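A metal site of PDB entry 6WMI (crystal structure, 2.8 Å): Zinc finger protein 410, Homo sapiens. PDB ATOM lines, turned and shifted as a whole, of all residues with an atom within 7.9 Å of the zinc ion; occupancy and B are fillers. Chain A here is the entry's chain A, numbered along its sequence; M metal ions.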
ATOM      1  N   GLN A 129      -7.448  -0.854   9.588  1.00  0.00           N
ATOM      2  CA  GLN A 129      -6.588   0.323   9.635  1.00  0.00           C
ATOM      3  C   GLN A 129      -7.421   1.586   9.786  1.00  0.00           C
ATOM      4  O   GLN A 129      -8.585   1.641   9.378  1.00  0.00           O
ATOM      5  CB  GLN A 129      -5.720   0.416   8.375  1.00  0.00           C
ATOM      6  CG  GLN A 129      -4.606   1.447   8.448  1.00  0.00           C
ATOM      7  CD  GLN A 129      -3.990   1.762   7.086  1.00  0.00           C
ATOM      8  OE1 GLN A 129      -4.597   1.501   6.045  1.00  0.00           O
ATOM      9  NE2 GLN A 129      -2.788   2.325   7.097  1.00  0.00           N
ATOM     10  N   CYS A 130      -6.819   2.611  10.391  1.00  0.00           N
ATOM     11  CA  CYS A 130      -7.403   3.941  10.445  1.00  0.00           C
ATOM     12  C   CYS A 130      -6.868   4.757   9.281  1.00  0.00           C
ATOM     13  O   CYS A 130      -5.657   4.933   9.130  1.00  0.00           O
ATOM     14  CB  CYS A 130      -7.076   4.627  11.778  1.00  0.00           C
ATOM     15  SG  CYS A 130      -7.553   6.384  11.874  1.00  0.00           S
ATOM     16  N   GLN A 131      -7.787   5.262   8.441  1.00  0.00           N
ATOM     17  CA  GLN A 131      -7.395   6.028   7.259  1.00  0.00           C
ATOM     18  C   GLN A 131      -6.787   7.386   7.619  1.00  0.00           C
ATOM     19  O   GLN A 131      -6.187   8.020   6.740  1.00  0.00           O
ATOM     20  CB  GLN A 131      -8.602   6.222   6.334  1.00  0.00           C
ATOM     21  N   VAL A 132      -6.931   7.840   8.869  1.00  0.00           N
ATOM     22  CA  VAL A 132      -6.453   9.166   9.266  1.00  0.00           C
ATOM     23  C   VAL A 132      -5.069   9.076   9.892  1.00  0.00           C
ATOM     24  O   VAL A 132      -4.115   9.659   9.375  1.00  0.00           O
ATOM     25  CB  VAL A 132      -7.452   9.832  10.240  1.00  0.00           C
ATOM     26  N   CYS A 133      -4.946   8.351  11.011  1.00  0.00           N
ATOM     27  CA  CYS A 133      -3.697   8.300  11.769  1.00  0.00           C
ATOM     28  C   CYS A 133      -2.780   7.165  11.324  1.00  0.00           C
ATOM     29  O   CYS A 133      -1.559   7.348  11.287  1.00  0.00           O
ATOM     30  CB  CYS A 133      -3.982   8.163  13.267  1.00  0.00           C
ATOM     31  SG  CYS A 133      -4.684   6.563  13.782  1.00  0.00           S
ATOM     32  N   GLY A 134      -3.340   6.015  10.994  1.00  0.00           N
ATOM     33  CA  GLY A 134      -2.560   4.845  10.625  1.00  0.00           C
ATOM     34  C   GLY A 134      -2.501   3.772  11.684  1.00  0.00           C
ATOM     35  O   GLY A 134      -1.852   2.741  11.454  1.00  0.00           O
ATOM     36  N   LYS A 135      -3.143   3.967  12.835  1.00  0.00           N
ATOM     37  CA  LYS A 135      -3.171   2.948  13.872  1.00  0.00           C
ATOM     38  C   LYS A 135      -3.841   1.680  13.344  1.00  0.00           C
ATOM     39  O   LYS A 135      -4.638   1.703  12.408  1.00  0.00           O
ATOM     40  CB  LYS A 135      -3.887   3.452  15.119  1.00  0.00           C
ATOM     41  N   THR A 136      -3.504   0.559  13.970  1.00  0.00           N
ATOM     42  CA  THR A 136      -3.909  -0.750  13.484  1.00  0.00           C
ATOM     43  C   THR A 136      -4.654  -1.478  14.598  1.00  0.00           C
ATOM     44  O   THR A 136      -4.202  -1.508  15.750  1.00  0.00           O
ATOM     45  CB  THR A 136      -2.662  -1.511  12.974  1.00  0.00           C
ATOM     46  OG1 THR A 136      -3.063  -2.631  12.174  1.00  0.00           O
ATOM     47  CG2 THR A 136      -1.733  -1.963  14.112  1.00  0.00           C
ATOM     48  N   PHE A 137      -5.830  -2.036  14.257  1.00  0.00           N
ATOM     49  CA  PHE A 137      -6.767  -2.530  15.259  1.00  0.00           C
ATOM     50  C   PHE A 137      -7.149  -3.973  14.984  1.00  0.00           C
ATOM     51  O   PHE A 137      -7.130  -4.435  13.834  1.00  0.00           O
ATOM     52  CB  PHE A 137      -8.052  -1.675  15.291  1.00  0.00           C
ATOM     53  CG  PHE A 137      -7.817  -0.256  15.713  1.00  0.00           C
ATOM     54  CD1 PHE A 137      -8.058   0.142  17.014  1.00  0.00           C
ATOM     55  CD2 PHE A 137      -7.347   0.675  14.797  1.00  0.00           C
ATOM     56  CE1 PHE A 137      -7.839   1.449  17.407  1.00  0.00           C
ATOM     57  CE2 PHE A 137      -7.127   1.983  15.190  1.00  0.00           C
ATOM     58  CZ  PHE A 137      -7.369   2.367  16.490  1.00  0.00           C
ATOM     59  N   ARG A 143     -11.724   0.011  15.502  1.00  0.00           N
ATOM     60  CA  ARG A 143     -11.313   1.065  14.593  1.00  0.00           C
ATOM     61  C   ARG A 143     -12.336   2.191  14.552  1.00  0.00           C
ATOM     62  O   ARG A 143     -11.983   3.367  14.452  1.00  0.00           O
ATOM     63  CB  ARG A 143     -11.085   0.483  13.188  1.00  0.00           C
ATOM     64  CG  ARG A 143     -10.596   1.485  12.137  1.00  0.00           C
ATOM     65  CD  ARG A 143     -11.713   1.924  11.220  1.00  0.00           C
ATOM     66  NE  ARG A 143     -12.415   0.781  10.622  1.00  0.00           N
ATOM     67  CZ  ARG A 143     -12.066   0.200   9.481  1.00  0.00           C
ATOM     68  NH1 ARG A 143     -11.019   0.648   8.800  1.00  0.00           N
ATOM     69  NH2 ARG A 143     -12.762  -0.830   9.013  1.00  0.00           N
ATOM     70  N   HIS A 146     -12.311   4.511  17.648  1.00  0.00           N
ATOM     71  CA  HIS A 146     -11.189   5.434  17.513  1.00  0.00           C
ATOM     72  C   HIS A 146     -11.505   6.535  16.504  1.00  0.00           C
ATOM     73  O   HIS A 146     -10.999   7.657  16.630  1.00  0.00           O
ATOM     74  CB  HIS A 146      -9.923   4.673  17.107  1.00  0.00           C
ATOM     75  CG  HIS A 146      -8.766   5.551  16.752  1.00  0.00           C
ATOM     76  ND1 HIS A 146      -7.894   6.042  17.688  1.00  0.00           N
ATOM     77  CD2 HIS A 146      -8.337   6.012  15.560  1.00  0.00           C
ATOM     78  CE1 HIS A 146      -6.977   6.774  17.092  1.00  0.00           C
ATOM     79  NE2 HIS A 146      -7.219   6.778  15.791  1.00  0.00           N
ATOM     80  N   MET A 147     -12.328   6.231  15.494  1.00  0.00           N
ATOM     81  CA  MET A 147     -12.767   7.255  14.551  1.00  0.00           C
ATOM     82  C   MET A 147     -13.707   8.256  15.229  1.00  0.00           C
ATOM     83  O   MET A 147     -13.659   9.449  14.936  1.00  0.00           O
ATOM     84  CB  MET A 147     -13.457   6.617  13.343  1.00  0.00           C
ATOM     85  CG  MET A 147     -12.532   5.808  12.430  1.00  0.00           C
ATOM     86  SD  MET A 147     -11.329   6.810  11.531  1.00  0.00           S
ATOM     87  CE  MET A 147     -10.753   5.615  10.314  1.00  0.00           C
ATOM     88  N   LYS A 149     -13.371   9.089  18.226  1.00  0.00           N
ATOM     89  CA  LYS A 149     -12.463   9.921  19.004  1.00  0.00           C
ATOM     90  C   LYS A 149     -11.850  11.028  18.142  1.00  0.00           C
ATOM     91  O   LYS A 149     -11.566  12.121  18.646  1.00  0.00           O
ATOM     92  CB  LYS A 149     -11.370   9.054  19.640  1.00  0.00           C
ATOM     93  CG  LYS A 149     -10.403   9.791  20.555  1.00  0.00           C
ATOM     94  CD  LYS A 149      -9.128  10.212  19.829  1.00  0.00           C
ATOM     95  CE  LYS A 149      -8.256   9.018  19.465  1.00  0.00           C
ATOM     96  NZ  LYS A 149      -7.523   8.472  20.636  1.00  0.00           N
ATOM     97  N   HIS A 150     -11.632  10.758  16.844  1.00  0.00           N
ATOM     98  CA  HIS A 150     -11.061  11.770  15.950  1.00  0.00           C
ATOM     99  C   HIS A 150     -12.038  12.901  15.683  1.00  0.00           C
ATOM    100  O   HIS A 150     -11.762  14.062  15.997  1.00  0.00           O
ATOM    101  CB  HIS A 150     -10.629  11.110  14.636  1.00  0.00           C
ATOM    102  CG  HIS A 150      -9.251  10.547  14.646  1.00  0.00           C
ATOM    103  ND1 HIS A 150      -8.368  10.748  15.691  1.00  0.00           N
ATOM    104  CD2 HIS A 150      -8.584   9.790  13.743  1.00  0.00           C
ATOM    105  CE1 HIS A 150      -7.233  10.139  15.423  1.00  0.00           C
ATOM    106  NE2 HIS A 150      -7.333   9.541  14.257  1.00  0.00           N
HETATM  107 ZN    ZN M   1      -6.869   7.573  13.923  1.00  0.00          ZN
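Of the 14 residues printed, 4 come within 4 Å of the zinc ion.
The nearest printed residue that does not touch the zinc ion is Val 132 (4.4 Å).
The zinc ion is bound by a ring nitrogen (NE2) of His 150, a ring nitrogen (NE2) of His 146, the side-chain sulfur (SG) of Cys 133 and the side-chain sulfur (SG) of Cys 130.
The zinc ion has four donor atoms within binding distance.
The side-chain sulfur (SG) of Cys 133 lies close to the backbone NH (N) of Lys 135.
The side-chain sulfur of Cys 130 lies close to the backbone NH of Val 132 (3.4 Å).
The backbone carbonyl oxygen (O) of Lys 135 is in hydrogen-bond range of the backbone NH (N) of Cys 130 (3.1 Å).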
